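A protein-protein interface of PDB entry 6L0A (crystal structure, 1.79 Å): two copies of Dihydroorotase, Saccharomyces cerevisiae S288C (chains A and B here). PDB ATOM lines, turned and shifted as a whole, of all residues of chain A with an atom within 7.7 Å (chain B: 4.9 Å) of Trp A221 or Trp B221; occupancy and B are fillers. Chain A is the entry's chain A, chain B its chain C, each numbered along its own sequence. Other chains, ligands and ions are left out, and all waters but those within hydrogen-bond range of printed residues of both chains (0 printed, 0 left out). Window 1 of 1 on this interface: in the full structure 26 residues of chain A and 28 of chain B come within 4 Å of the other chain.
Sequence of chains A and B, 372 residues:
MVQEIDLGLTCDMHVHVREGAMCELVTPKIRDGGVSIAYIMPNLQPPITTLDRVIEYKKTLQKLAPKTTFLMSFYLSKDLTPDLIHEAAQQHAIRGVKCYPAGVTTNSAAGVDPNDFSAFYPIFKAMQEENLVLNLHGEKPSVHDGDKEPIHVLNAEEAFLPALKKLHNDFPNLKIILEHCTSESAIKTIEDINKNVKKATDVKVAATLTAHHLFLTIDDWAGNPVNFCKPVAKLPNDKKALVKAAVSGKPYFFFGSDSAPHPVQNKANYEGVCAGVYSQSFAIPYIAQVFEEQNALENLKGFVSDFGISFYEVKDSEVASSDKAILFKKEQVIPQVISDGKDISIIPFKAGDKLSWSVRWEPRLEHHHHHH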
ATOM      1  N   VAL A 153     -25.533  15.985 -20.080  1.00  0.00           N
ATOM      2  CA  VAL A 153     -25.644  14.862 -19.153  1.00  0.00           C
ATOM      3  C   VAL A 153     -26.619  15.141 -18.016  1.00  0.00           C
ATOM      4  O   VAL A 153     -27.081  14.199 -17.364  1.00  0.00           O
ATOM      5  CB  VAL A 153     -24.257  14.455 -18.583  1.00  0.00           C
ATOM      6  CG1 VAL A 153     -23.363  13.907 -19.682  1.00  0.00           C
ATOM      7  CG2 VAL A 153     -23.600  15.617 -17.866  1.00  0.00           C
ATOM      8  N   LEU A 154     -26.951  16.400 -17.740  1.00  0.00           N
ATOM      9  CA  LEU A 154     -27.869  16.643 -16.634  1.00  0.00           C
ATOM     10  C   LEU A 154     -29.336  16.584 -17.043  1.00  0.00           C
ATOM     11  O   LEU A 154     -30.179  16.265 -16.201  1.00  0.00           O
ATOM     12  CB  LEU A 154     -27.576  17.993 -15.980  1.00  0.00           C
ATOM     13  CG  LEU A 154     -26.206  17.996 -15.305  1.00  0.00           C
ATOM     14  CD1 LEU A 154     -25.942  19.383 -14.809  1.00  0.00           C
ATOM     15  CD2 LEU A 154     -26.140  16.980 -14.174  1.00  0.00           C
ATOM     16  N   HIS A 213     -27.325   5.783  -6.636  1.00  0.00           N
ATOM     17  CA  HIS A 213     -28.060   7.038  -6.814  1.00  0.00           C
ATOM     18  C   HIS A 213     -28.901   7.406  -5.593  1.00  0.00           C
ATOM     19  O   HIS A 213     -29.405   8.532  -5.528  1.00  0.00           O
ATOM     20  CB  HIS A 213     -28.941   6.975  -8.060  1.00  0.00           C
ATOM     21  CG  HIS A 213     -28.161   6.982  -9.341  1.00  0.00           C
ATOM     22  ND1 HIS A 213     -28.031   5.868 -10.138  1.00  0.00           N
ATOM     23  CD2 HIS A 213     -27.469   7.969  -9.960  1.00  0.00           C
ATOM     24  CE1 HIS A 213     -27.314   6.168 -11.206  1.00  0.00           C
ATOM     25  NE2 HIS A 213     -26.941   7.432 -11.112  1.00  0.00           N
ATOM     26  N   LEU A 216     -25.542   9.436  -3.947  1.00  0.00           N
ATOM     27  CA  LEU A 216     -24.656  10.358  -4.649  1.00  0.00           C
ATOM     28  C   LEU A 216     -25.390  11.563  -5.210  1.00  0.00           C
ATOM     29  O   LEU A 216     -26.550  11.477  -5.630  1.00  0.00           O
ATOM     30  CB  LEU A 216     -23.957   9.667  -5.817  1.00  0.00           C
ATOM     31  CG  LEU A 216     -23.073   8.464  -5.518  1.00  0.00           C
ATOM     32  CD1 LEU A 216     -22.637   7.852  -6.843  1.00  0.00           C
ATOM     33  CD2 LEU A 216     -21.878   8.875  -4.688  1.00  0.00           C
ATOM     34  N   THR A 217     -24.665  12.682  -5.273  1.00  0.00           N
ATOM     35  CA  THR A 217     -25.019  13.816  -6.115  1.00  0.00           C
ATOM     36  C   THR A 217     -23.790  14.209  -6.929  1.00  0.00           C
ATOM     37  O   THR A 217     -22.699  13.646  -6.763  1.00  0.00           O
ATOM     38  CB  THR A 217     -25.496  15.024  -5.299  1.00  0.00           C
ATOM     39  OG1 THR A 217     -24.400  15.504  -4.510  1.00  0.00           O
ATOM     40  CG2 THR A 217     -26.683  14.650  -4.395  1.00  0.00           C
ATOM     41  N   ILE A 218     -23.966  15.224  -7.782  1.00  0.00           N
ATOM     42  CA  ILE A 218     -22.884  15.695  -8.644  1.00  0.00           C
ATOM     43  C   ILE A 218     -21.618  16.001  -7.850  1.00  0.00           C
ATOM     44  O   ILE A 218     -20.505  15.773  -8.342  1.00  0.00           O
ATOM     45  CB  ILE A 218     -23.355  16.921  -9.465  1.00  0.00           C
ATOM     46  CG1 ILE A 218     -22.270  17.345 -10.456  1.00  0.00           C
ATOM     47  CG2 ILE A 218     -23.798  18.068  -8.541  1.00  0.00           C
ATOM     48  CD1 ILE A 218     -22.796  18.209 -11.588  1.00  0.00           C
ATOM     49  N   ASP A 219     -21.748  16.485  -6.612  1.00  0.00           N
ATOM     50  CA  ASP A 219     -20.543  16.814  -5.849  1.00  0.00           C
ATOM     51  C   ASP A 219     -19.685  15.586  -5.584  1.00  0.00           C
ATOM     52  O   ASP A 219     -18.460  15.696  -5.437  1.00  0.00           O
ATOM     53  CB  ASP A 219     -20.910  17.474  -4.530  1.00  0.00           C
ATOM     54  CG  ASP A 219     -21.021  18.970  -4.653  1.00  0.00           C
ATOM     55  OD1 ASP A 219     -21.163  19.445  -5.794  1.00  0.00           O
ATOM     56  OD2 ASP A 219     -20.965  19.659  -3.614  1.00  0.00           O
ATOM     57  N   ASP A 220     -20.304  14.413  -5.515  1.00  0.00           N
ATOM     58  CA  ASP A 220     -19.571  13.192  -5.211  1.00  0.00           C
ATOM     59  C   ASP A 220     -18.731  12.674  -6.365  1.00  0.00           C
ATOM     60  O   ASP A 220     -17.767  11.940  -6.109  1.00  0.00           O
ATOM     61  CB  ASP A 220     -20.546  12.099  -4.775  1.00  0.00           C
ATOM     62  CG  ASP A 220     -21.239  12.426  -3.482  1.00  0.00           C
ATOM     63  OD1 ASP A 220     -20.532  12.629  -2.473  1.00  0.00           O
ATOM     64  OD2 ASP A 220     -22.488  12.495  -3.459  1.00  0.00           O
ATOM     65  N   TRP A 221     -19.075  12.980  -7.627  1.00  0.00           N
ATOM     66  CA  TRP A 221     -18.255  12.511  -8.735  1.00  0.00           C
ATOM     67  C   TRP A 221     -17.466  13.624  -9.420  1.00  0.00           C
ATOM     68  O   TRP A 221     -16.596  13.316 -10.240  1.00  0.00           O
ATOM     69  CB  TRP A 221     -19.099  11.739  -9.774  1.00  0.00           C
ATOM     70  CG  TRP A 221     -20.263  12.483 -10.401  1.00  0.00           C
ATOM     71  CD1 TRP A 221     -21.565  12.505  -9.958  1.00  0.00           C
ATOM     72  CD2 TRP A 221     -20.237  13.274 -11.599  1.00  0.00           C
ATOM     73  NE1 TRP A 221     -22.339  13.271 -10.809  1.00  0.00           N
ATOM     74  CE2 TRP A 221     -21.549  13.755 -11.818  1.00  0.00           C
ATOM     75  CE3 TRP A 221     -19.226  13.637 -12.501  1.00  0.00           C
ATOM     76  CZ2 TRP A 221     -21.863  14.595 -12.886  1.00  0.00           C
ATOM     77  CZ3 TRP A 221     -19.549  14.440 -13.567  1.00  0.00           C
ATOM     78  CH2 TRP A 221     -20.850  14.913 -13.753  1.00  0.00           C
ATOM     79  N   ALA A 222     -17.719  14.896  -9.088  1.00  0.00           N
ATOM     80  CA  ALA A 222     -16.901  15.993  -9.591  1.00  0.00           C
ATOM     81  C   ALA A 222     -15.522  15.876  -8.954  1.00  0.00           C
ATOM     82  O   ALA A 222     -15.333  16.193  -7.776  1.00  0.00           O
ATOM     83  CB  ALA A 222     -17.536  17.348  -9.283  1.00  0.00           C
ATOM     84  N   GLY A 223     -14.568  15.396  -9.721  1.00  0.00           N
ATOM     85  CA  GLY A 223     -13.239  15.118  -9.215  1.00  0.00           C
ATOM     86  C   GLY A 223     -13.003  13.680  -8.804  1.00  0.00           C
ATOM     87  O   GLY A 223     -11.854  13.318  -8.501  1.00  0.00           O
ATOM     88  N   ASN A 224     -14.045  12.839  -8.787  1.00  0.00           N
ATOM     89  CA  ASN A 224     -13.915  11.452  -8.328  1.00  0.00           C
ATOM     90  C   ASN A 224     -14.480  10.499  -9.368  1.00  0.00           C
ATOM     91  O   ASN A 224     -15.654  10.102  -9.280  1.00  0.00           O
ATOM     92  CB  ASN A 224     -14.624  11.244  -6.996  1.00  0.00           C
ATOM     93  CG  ASN A 224     -14.109  12.163  -5.904  1.00  0.00           C
ATOM     94  OD1 ASN A 224     -12.900  12.347  -5.742  1.00  0.00           O
ATOM     95  ND2 ASN A 224     -15.028  12.732  -5.134  1.00  0.00           N
ATOM     96  N   PRO A 225     -13.672  10.090 -10.347  1.00  0.00           N
ATOM     97  CA  PRO A 225     -14.154   9.129 -11.351  1.00  0.00           C
ATOM     98  C   PRO A 225     -14.757   7.859 -10.774  1.00  0.00           C
ATOM     99  O   PRO A 225     -15.628   7.267 -11.424  1.00  0.00           O
ATOM    100  CB  PRO A 225     -12.887   8.833 -12.168  1.00  0.00           C
ATOM    101  CG  PRO A 225     -12.117  10.112 -12.095  1.00  0.00           C
ATOM    102  CD  PRO A 225     -12.314  10.578 -10.675  1.00  0.00           C
ATOM    103  N   VAL A 226     -14.357   7.442  -9.570  1.00  0.00           N
ATOM    104  CA  VAL A 226     -14.906   6.227  -8.975  1.00  0.00           C
ATOM    105  C   VAL A 226     -16.414   6.328  -8.749  1.00  0.00           C
ATOM    106  O   VAL A 226     -17.100   5.302  -8.658  1.00  0.00           O
ATOM    107  CB  VAL A 226     -14.170   5.897  -7.649  1.00  0.00           C
ATOM    108  CG1 VAL A 226     -14.587   6.836  -6.531  1.00  0.00           C
ATOM    109  CG2 VAL A 226     -14.421   4.444  -7.247  1.00  0.00           C
ATOM    110  N   ASN A 227     -16.951   7.544  -8.653  1.00  0.00           N
ATOM    111  CA  ASN A 227     -18.383   7.748  -8.485  1.00  0.00           C
ATOM    112  C   ASN A 227     -19.072   8.182  -9.771  1.00  0.00           C
ATOM    113  O   ASN A 227     -20.249   8.566  -9.734  1.00  0.00           O
ATOM    114  CB  ASN A 227     -18.631   8.789  -7.397  1.00  0.00           C
ATOM    115  CG  ASN A 227     -18.257   8.275  -6.022  1.00  0.00           C
ATOM    116  OD1 ASN A 227     -18.416   7.091  -5.745  1.00  0.00           O
ATOM    117  ND2 ASN A 227     -17.752   9.160  -5.160  1.00  0.00           N
ATOM    118  N   PHE A 228     -18.357   8.163 -10.890  1.00  0.00           N
ATOM    119  CA  PHE A 228     -18.910   8.569 -12.174  1.00  0.00           C
ATOM    120  C   PHE A 228     -19.573   7.367 -12.831  1.00  0.00           C
ATOM    121  O   PHE A 228     -18.927   6.332 -13.031  1.00  0.00           O
ATOM    122  CB  PHE A 228     -17.810   9.123 -13.080  1.00  0.00           C
ATOM    123  CG  PHE A 228     -18.212   9.265 -14.528  1.00  0.00           C
ATOM    124  CD1 PHE A 228     -19.233  10.126 -14.893  1.00  0.00           C
ATOM    125  CD2 PHE A 228     -17.561   8.541 -15.521  1.00  0.00           C
ATOM    126  CE1 PHE A 228     -19.596  10.270 -16.233  1.00  0.00           C
ATOM    127  CE2 PHE A 228     -17.921   8.675 -16.856  1.00  0.00           C
ATOM    128  CZ  PHE A 228     -18.946   9.541 -17.211  1.00  0.00           C
ATOM    129  N   CYS A 229     -20.846   7.522 -13.192  1.00  0.00           N
ATOM    130  CA  CYS A 229     -21.588   6.478 -13.876  1.00  0.00           C
ATOM    131  C   CYS A 229     -22.578   7.163 -14.801  1.00  0.00           C
ATOM    132  O   CYS A 229     -22.730   8.381 -14.762  1.00  0.00           O
ATOM    133  CB  CYS A 229     -22.326   5.586 -12.877  1.00  0.00           C
ATOM    134  SG  CYS A 229     -23.540   6.525 -11.904  1.00  0.00           S
ATOM    135  N   PRO A 231     -26.771   6.915 -15.923  1.00  0.00           N
ATOM    136  CA  PRO A 231     -26.843   8.376 -16.012  1.00  0.00           C
ATOM    137  C   PRO A 231     -26.148   8.950 -14.794  1.00  0.00           C
ATOM    138  O   PRO A 231     -26.073   8.301 -13.759  1.00  0.00           O
ATOM    139  CB  PRO A 231     -28.353   8.687 -15.981  1.00  0.00           C
ATOM    140  CG  PRO A 231     -29.053   7.329 -16.145  1.00  0.00           C
ATOM    141  CD  PRO A 231     -28.071   6.312 -15.594  1.00  0.00           C
ATOM    142  N   VAL A 232     -25.606  10.149 -14.950  1.00  0.00           N
ATOM    143  CA  VAL A 232     -24.796  10.739 -13.905  1.00  0.00           C
ATOM    144  C   VAL A 232     -25.668  11.097 -12.686  1.00  0.00           C
ATOM    145  O   VAL A 232     -26.858  11.380 -12.820  1.00  0.00           O
ATOM    146  CB  VAL A 232     -24.128  11.955 -14.573  1.00  0.00           C
ATOM    147  CG1 VAL A 232     -25.005  13.223 -14.563  1.00  0.00           C
ATOM    148  CG2 VAL A 232     -22.708  12.082 -14.249  1.00  0.00           C
ATOM    149  N   ALA A 233     -25.082  11.036 -11.479  1.00  0.00           N
ATOM    150  CA  ALA A 233     -25.822  11.493 -10.298  1.00  0.00           C
ATOM    151  C   ALA A 233     -26.015  13.007 -10.371  1.00  0.00           C
ATOM    152  O   ALA A 233     -25.101  13.750 -10.741  1.00  0.00           O
ATOM    153  CB  ALA A 233     -25.100  11.118  -8.997  1.00  0.00           C
ATOM    154  N   LYS A 234     -27.203  13.470 -10.011  1.00  0.00           N
ATOM    155  CA  LYS A 234     -27.651  14.815 -10.372  1.00  0.00           C
ATOM    156  C   LYS A 234     -27.724  15.679  -9.110  1.00  0.00           C
ATOM    157  O   LYS A 234     -26.756  15.680  -8.343  1.00  0.00           O
ATOM    158  CB  LYS A 234     -28.938  14.720 -11.177  1.00  0.00           C
ATOM    159  CG  LYS A 234     -28.698  14.015 -12.531  1.00  0.00           C
ATOM    160  CD  LYS A 234     -29.988  13.777 -13.309  1.00  0.00           C
ATOM    161  CE  LYS A 234     -29.666  13.329 -14.731  1.00  0.00           C
ATOM    162  NZ  LYS A 234     -28.912  12.029 -14.726  1.00  0.00           N
ATOM    163  N   LEU A 235     -28.786  16.433  -8.888  1.00  0.00           N
ATOM    164  CA  LEU A 235     -28.779  17.430  -7.822  1.00  0.00           C
ATOM    165  C   LEU A 235     -29.437  16.897  -6.555  1.00  0.00           C
ATOM    166  O   LEU A 235     -30.129  15.876  -6.581  1.00  0.00           O
ATOM    167  CB  LEU A 235     -29.510  18.687  -8.294  1.00  0.00           C
ATOM    168  CG  LEU A 235     -28.967  19.250  -9.607  1.00  0.00           C
ATOM    169  CD1 LEU A 235     -29.648  20.573  -9.936  1.00  0.00           C
ATOM    170  CD2 LEU A 235     -27.447  19.407  -9.532  1.00  0.00           C
ATOM    171  N   TYR A 270      -6.821   9.749 -17.435  1.00  0.00           N
ATOM    172  CA  TYR A 270      -6.950  11.199 -17.526  1.00  0.00           C
ATOM    173  C   TYR A 270      -7.945  11.623 -18.591  1.00  0.00           C
ATOM    174  O   TYR A 270      -8.410  12.769 -18.563  1.00  0.00           O
ATOM    175  CB  TYR A 270      -5.587  11.865 -17.738  1.00  0.00           C
ATOM    176  CG  TYR A 270      -4.885  11.612 -19.055  1.00  0.00           C
ATOM    177  CD1 TYR A 270      -5.242  12.302 -20.204  1.00  0.00           C
ATOM    178  CD2 TYR A 270      -3.824  10.723 -19.126  1.00  0.00           C
ATOM    179  CE1 TYR A 270      -4.582  12.088 -21.398  1.00  0.00           C
ATOM    180  CE2 TYR A 270      -3.155  10.507 -20.314  1.00  0.00           C
ATOM    181  CZ  TYR A 270      -3.534  11.191 -21.442  1.00  0.00           C
ATOM    182  OH  TYR A 270      -2.863  10.968 -22.626  1.00  0.00           O
ATOM    183  N   VAL A 273     -12.561   8.074 -18.941  1.00  0.00           N
ATOM    184  CA  VAL A 273     -12.847   7.248 -17.773  1.00  0.00           C
ATOM    185  C   VAL A 273     -14.072   6.390 -18.052  1.00  0.00           C
ATOM    186  O   VAL A 273     -15.073   6.871 -18.598  1.00  0.00           O
ATOM    187  CB  VAL A 273     -13.083   8.142 -16.539  1.00  0.00           C
ATOM    188  CG1 VAL A 273     -13.854   7.375 -15.451  1.00  0.00           C
ATOM    189  CG2 VAL A 273     -11.769   8.670 -15.991  1.00  0.00           C
ATOM    190  N   VAL A 277     -20.307   2.190 -11.387  1.00  0.00           N
ATOM    191  CA  VAL A 277     -20.056   2.041  -9.956  1.00  0.00           C
ATOM    192  C   VAL A 277     -20.234   0.572  -9.615  1.00  0.00           C
ATOM    193  O   VAL A 277     -21.176  -0.061 -10.096  1.00  0.00           O
ATOM    194  CB  VAL A 277     -21.018   2.916  -9.123  1.00  0.00           C
ATOM    195  CG1 VAL A 277     -20.997   2.524  -7.628  1.00  0.00           C
ATOM    196  CG2 VAL A 277     -20.686   4.402  -9.308  1.00  0.00           C
ATOM    197  N   THR B 217     -18.203  22.364 -21.747  1.00  0.00           N
ATOM    198  CA  THR B 217     -19.441  22.244 -21.004  1.00  0.00           C
ATOM    199  C   THR B 217     -19.296  21.019 -20.109  1.00  0.00           C
ATOM    200  O   THR B 217     -18.316  20.286 -20.210  1.00  0.00           O
ATOM    201  CB  THR B 217     -20.622  22.117 -21.965  1.00  0.00           C
ATOM    202  OG1 THR B 217     -21.821  22.523 -21.305  1.00  0.00           O
ATOM    203  CG2 THR B 217     -20.743  20.710 -22.426  1.00  0.00           C
ATOM    204  N   ILE B 218     -20.281  20.779 -19.234  1.00  0.00           N
ATOM    205  CA  ILE B 218     -20.197  19.637 -18.318  1.00  0.00           C
ATOM    206  C   ILE B 218     -19.981  18.323 -19.071  1.00  0.00           C
ATOM    207  O   ILE B 218     -19.301  17.419 -18.573  1.00  0.00           O
ATOM    208  CB  ILE B 218     -21.456  19.580 -17.427  1.00  0.00           C
ATOM    209  CG1 ILE B 218     -21.355  18.437 -16.415  1.00  0.00           C
ATOM    210  CG2 ILE B 218     -22.741  19.491 -18.278  1.00  0.00           C
ATOM    211  CD1 ILE B 218     -22.422  18.484 -15.342  1.00  0.00           C
ATOM    212  N   ASP B 219     -20.542  18.194 -20.278  1.00  0.00           N
ATOM    213  CA  ASP B 219     -20.360  16.960 -21.041  1.00  0.00           C
ATOM    214  C   ASP B 219     -18.898  16.673 -21.319  1.00  0.00           C
ATOM    215  O   ASP B 219     -18.513  15.511 -21.479  1.00  0.00           O
ATOM    216  CB  ASP B 219     -21.108  17.033 -22.373  1.00  0.00           C
ATOM    217  CG  ASP B 219     -22.568  16.751 -22.224  1.00  0.00           C
ATOM    218  OD1 ASP B 219     -23.120  17.049 -21.154  1.00  0.00           O
ATOM    219  OD2 ASP B 219     -23.173  16.257 -23.193  1.00  0.00           O
ATOM    220  N   ASP B 220     -18.074  17.707 -21.414  1.00  0.00           N
ATOM    221  CA  ASP B 220     -16.683  17.504 -21.794  1.00  0.00           C
ATOM    222  C   ASP B 220     -15.788  17.077 -20.645  1.00  0.00           C
ATOM    223  O   ASP B 220     -14.708  16.536 -20.905  1.00  0.00           O
ATOM    224  CB  ASP B 220     -16.120  18.782 -22.420  1.00  0.00           C
ATOM    225  CG  ASP B 220     -16.882  19.200 -23.650  1.00  0.00           C
ATOM    226  OD1 ASP B 220     -17.044  18.356 -24.555  1.00  0.00           O
ATOM    227  OD2 ASP B 220     -17.323  20.363 -23.722  1.00  0.00           O
ATOM    228  N   TRP B 221     -16.180  17.301 -19.384  1.00  0.00           N
ATOM    229  CA  TRP B 221     -15.338  16.844 -18.286  1.00  0.00           C
ATOM    230  C   TRP B 221     -15.932  15.698 -17.484  1.00  0.00           C
ATOM    231  O   TRP B 221     -15.208  15.102 -16.679  1.00  0.00           O
ATOM    232  CB  TRP B 221     -14.964  18.002 -17.331  1.00  0.00           C
ATOM    233  CG  TRP B 221     -16.107  18.697 -16.634  1.00  0.00           C
ATOM    234  CD1 TRP B 221     -16.712  19.859 -17.018  1.00  0.00           C
ATOM    235  CD2 TRP B 221     -16.745  18.300 -15.408  1.00  0.00           C
ATOM    236  NE1 TRP B 221     -17.709  20.194 -16.129  1.00  0.00           N
ATOM    237  CE2 TRP B 221     -17.742  19.263 -15.126  1.00  0.00           C
ATOM    238  CE3 TRP B 221     -16.564  17.227 -14.517  1.00  0.00           C
ATOM    239  CZ2 TRP B 221     -18.572  19.176 -14.005  1.00  0.00           C
ATOM    240  CZ3 TRP B 221     -17.384  17.146 -13.402  1.00  0.00           C
ATOM    241  CH2 TRP B 221     -18.373  18.109 -13.157  1.00  0.00           C
ATOM    242  N   ALA B 222     -17.194  15.328 -17.713  1.00  0.00           N
ATOM    243  CA  ALA B 222     -17.822  14.310 -16.866  1.00  0.00           C
ATOM    244  C   ALA B 222     -16.981  13.029 -16.790  1.00  0.00           C
ATOM    245  O   ALA B 222     -16.772  12.473 -15.706  1.00  0.00           O
ATOM    246  CB  ALA B 222     -19.235  14.010 -17.377  1.00  0.00           C
ATOM    247  N   GLY B 223     -16.480  12.559 -17.928  1.00  0.00           N
ATOM    248  CA  GLY B 223     -15.613  11.393 -17.955  1.00  0.00           C
ATOM    249  C   GLY B 223     -14.208  11.686 -18.445  1.00  0.00           C
ATOM    250  O   GLY B 223     -13.490  10.768 -18.856  1.00  0.00           O
ATOM    251  N   ASN B 224     -13.800  12.961 -18.402  1.00  0.00           N
ATOM    252  CA  ASN B 224     -12.490  13.407 -18.886  1.00  0.00           C
ATOM    253  C   ASN B 224     -11.831  14.272 -17.818  1.00  0.00           C
ATOM    254  O   ASN B 224     -11.996  15.503 -17.812  1.00  0.00           O
ATOM    255  CB  ASN B 224     -12.614  14.184 -20.198  1.00  0.00           C
ATOM    256  CG  ASN B 224     -13.163  13.346 -21.343  1.00  0.00           C
ATOM    257  OD1 ASN B 224     -12.686  12.247 -21.612  1.00  0.00           O
ATOM    258  ND2 ASN B 224     -14.156  13.884 -22.043  1.00  0.00           N
ATOM    259  N   PRO B 225     -11.096  13.668 -16.886  1.00  0.00           N
ATOM    260  CA  PRO B 225     -10.440  14.468 -15.831  1.00  0.00           C
ATOM    261  C   PRO B 225      -9.562  15.597 -16.358  1.00  0.00           C
ATOM    262  O   PRO B 225      -9.403  16.613 -15.671  1.00  0.00           O
ATOM    263  CB  PRO B 225      -9.620  13.419 -15.077  1.00  0.00           C
ATOM    264  CG  PRO B 225     -10.440  12.163 -15.234  1.00  0.00           C
ATOM    265  CD  PRO B 225     -10.992  12.221 -16.626  1.00  0.00           C
ATOM    266  N   ASN B 227     -10.249  17.736 -18.471  1.00  0.00           N
ATOM    267  CA  ASN B 227     -11.072  18.928 -18.621  1.00  0.00           C
ATOM    268  C   ASN B 227     -11.726  19.376 -17.315  1.00  0.00           C
ATOM    269  O   ASN B 227     -12.513  20.317 -17.341  1.00  0.00           O
ATOM    270  CB  ASN B 227     -12.150  18.693 -19.684  1.00  0.00           C
ATOM    271  CG  ASN B 227     -11.576  18.630 -21.087  1.00  0.00           C
ATOM    272  OD1 ASN B 227     -10.562  19.274 -21.380  1.00  0.00           O
ATOM    273  ND2 ASN B 227     -12.210  17.843 -21.958  1.00  0.00           N
ATOM    274  N   PHE B 228     -11.442  18.720 -16.192  1.00  0.00           N
ATOM    275  CA  PHE B 228     -12.036  19.100 -14.912  1.00  0.00           C
ATOM    276  C   PHE B 228     -11.251  20.266 -14.320  1.00  0.00           C
ATOM    277  O   PHE B 228     -10.035  20.161 -14.156  1.00  0.00           O
ATOM    278  CB  PHE B 228     -12.029  17.900 -13.957  1.00  0.00           C
ATOM    279  CG  PHE B 228     -12.411  18.225 -12.541  1.00  0.00           C
ATOM    280  CD1 PHE B 228     -13.699  18.657 -12.235  1.00  0.00           C
ATOM    281  CD2 PHE B 228     -11.491  18.077 -11.501  1.00  0.00           C
ATOM    282  CE1 PHE B 228     -14.060  18.953 -10.922  1.00  0.00           C
ATOM    283  CE2 PHE B 228     -11.855  18.373 -10.175  1.00  0.00           C
ATOM    284  CZ  PHE B 228     -13.136  18.816  -9.891  1.00  0.00           C
ATOM    285  N   VAL B 232     -16.358  24.445 -12.267  1.00  0.00           N
ATOM    286  CA  VAL B 232     -16.543  23.483 -13.343  1.00  0.00           C
ATOM    287  C   VAL B 232     -17.244  24.165 -14.511  1.00  0.00           C
ATOM    288  O   VAL B 232     -18.011  25.119 -14.329  1.00  0.00           O
ATOM    289  CB  VAL B 232     -17.349  22.261 -12.857  1.00  0.00           C
ATOM    290  CG1 VAL B 232     -16.665  21.600 -11.645  1.00  0.00           C
ATOM    291  CG2 VAL B 232     -18.795  22.648 -12.535  1.00  0.00           C
ATOM    292  N   ALA B 233     -16.979  23.672 -15.720  1.00  0.00           N
ATOM    293  CA  ALA B 233     -17.753  24.091 -16.883  1.00  0.00           C
ATOM    294  C   ALA B 233     -19.188  23.597 -16.742  1.00  0.00           C
ATOM    295  O   ALA B 233     -19.430  22.468 -16.297  1.00  0.00           O
ATOM    296  CB  ALA B 233     -17.118  23.551 -18.170  1.00  0.00           C
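Ile B218 touches its own counterpart, Ile A218.
Trp A221 touches Ala B222, but with the chains exchanged Ala A222 does not touch Trp B221 (4.01 Å).
Ala A222 touches Phe B228, and with the chains exchanged Phe A228 touches Ala B222.
Gly A223 touches Phe B228, and with the chains exchanged Phe A228 touches Gly B223.
Positions printed for both chains: 217, 218, 219, 220, 221, 222, 223, 224, 225, 227, 228, 232 and 233.
Of the 14 pairs that touch across the chains among the printed residues, 6 have their exchanged pair printed and touching as well.
The backbone carbonyl oxygen of Ala A233 sits at hydrogen-bond distance from the indole nitrogen of Trp A221, 2.8 Å away.
N of Ile B218 sits at hydrogen-bond distance from O of Ala B233 (3.5 Å).
The backbone NH (N) of Ile A218 is in hydrogen-bond range of the backbone carbonyl oxygen (O) of Lys A234 (2.9 Å).
The backbone NH (N) of Ile A218 sits at hydrogen-bond distance from the backbone carbonyl oxygen (O) of Ala A233.
O of Asp B220 lies within hydrogen-bond range of ND2 of Asn B224 (2.9 Å).
The indole nitrogen (NE1) of Trp B221 sits at hydrogen-bond distance from the backbone carbonyl oxygen (O) of Ala B233.
Trp A221 touches just these residues of chain B: Trp B221 and Ala B222.
Printed residues of chain B within 4 Å of Ala A222: Phe B228.
Printed residues of chain B within 4 Å of Gly A223: Phe B228.
Asn A224 touches none of the printed residues of chain B.
Of the printed residues of chain A, Trp B221 touches Trp A221 (3.5 Å).
Of the printed residues of chain A, Phe B228 touches Ala A222 (3.9 Å) and Gly A223 (3.7 Å).
The nearest printed residue of chain A that does not touch Trp B221 is Ala A222 (4.01 Å).
The nearest printed residue of chain A that does not touch Phe B228 is Asn A224 (6.1 Å).
Of the 13 printed residues of chain B, 8 touch a printed residue of chain A.
Printed residues of chain B that touch a printed residue of chain A: Ile B218, Asp B219, Trp B221, Ala B222, Gly B223, Asn B224, Pro B225 and Phe B228.
Hydrophobic or aromatic side chains of chain B within 4 Å of the printed part of chain A: Ile B218, Trp B221, Ala B222, Pro B225 and Phe B228.
Along chain B the printed residues that touch a printed residue of chain A span positions 218 to 228.
Hydrophobic or aromatic side chains of chain A within 4 Å of the printed part of chain B: Val A153, Leu A154, Ile A218, Trp A221, Phe A228 and Val A273.
The backbone carbonyl oxygen (O) of Tyr A270 lies close to the backbone nitrogen (N) of Pro B225 (3.3 Å).
The backbone NH (N) of Val A273 lies within hydrogen-bond range of the backbone carbonyl oxygen (O) of Gly B223, 2.9 Å away.
The side-chain carboxylate (OD1) of Asp B219 sits at hydrogen-bond distance from the backbone NH (N) of Val A153, at 2.8 Å.
Leu A154 touches Ile B218 (CD1 to CD1, 3.7 Å).
Ile B218 touches Ile A218.
Trp B221 touches Trp A221 (CZ3 to CZ3, 3.5 Å).
Ala B222 touches Trp A221 (CA to CZ3, 3.7 Å).
CZ of Phe B228 touches C of Ala A222, 3.9 Å away.
Phe B228 touches Gly A223 (CE2 to CA, 3.7 Å).
Phe A228 touches Ala B222.
Gly B223 touches Phe A228.
Asn B224 touches Tyr A270.
Pro B225 touches Val A273.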
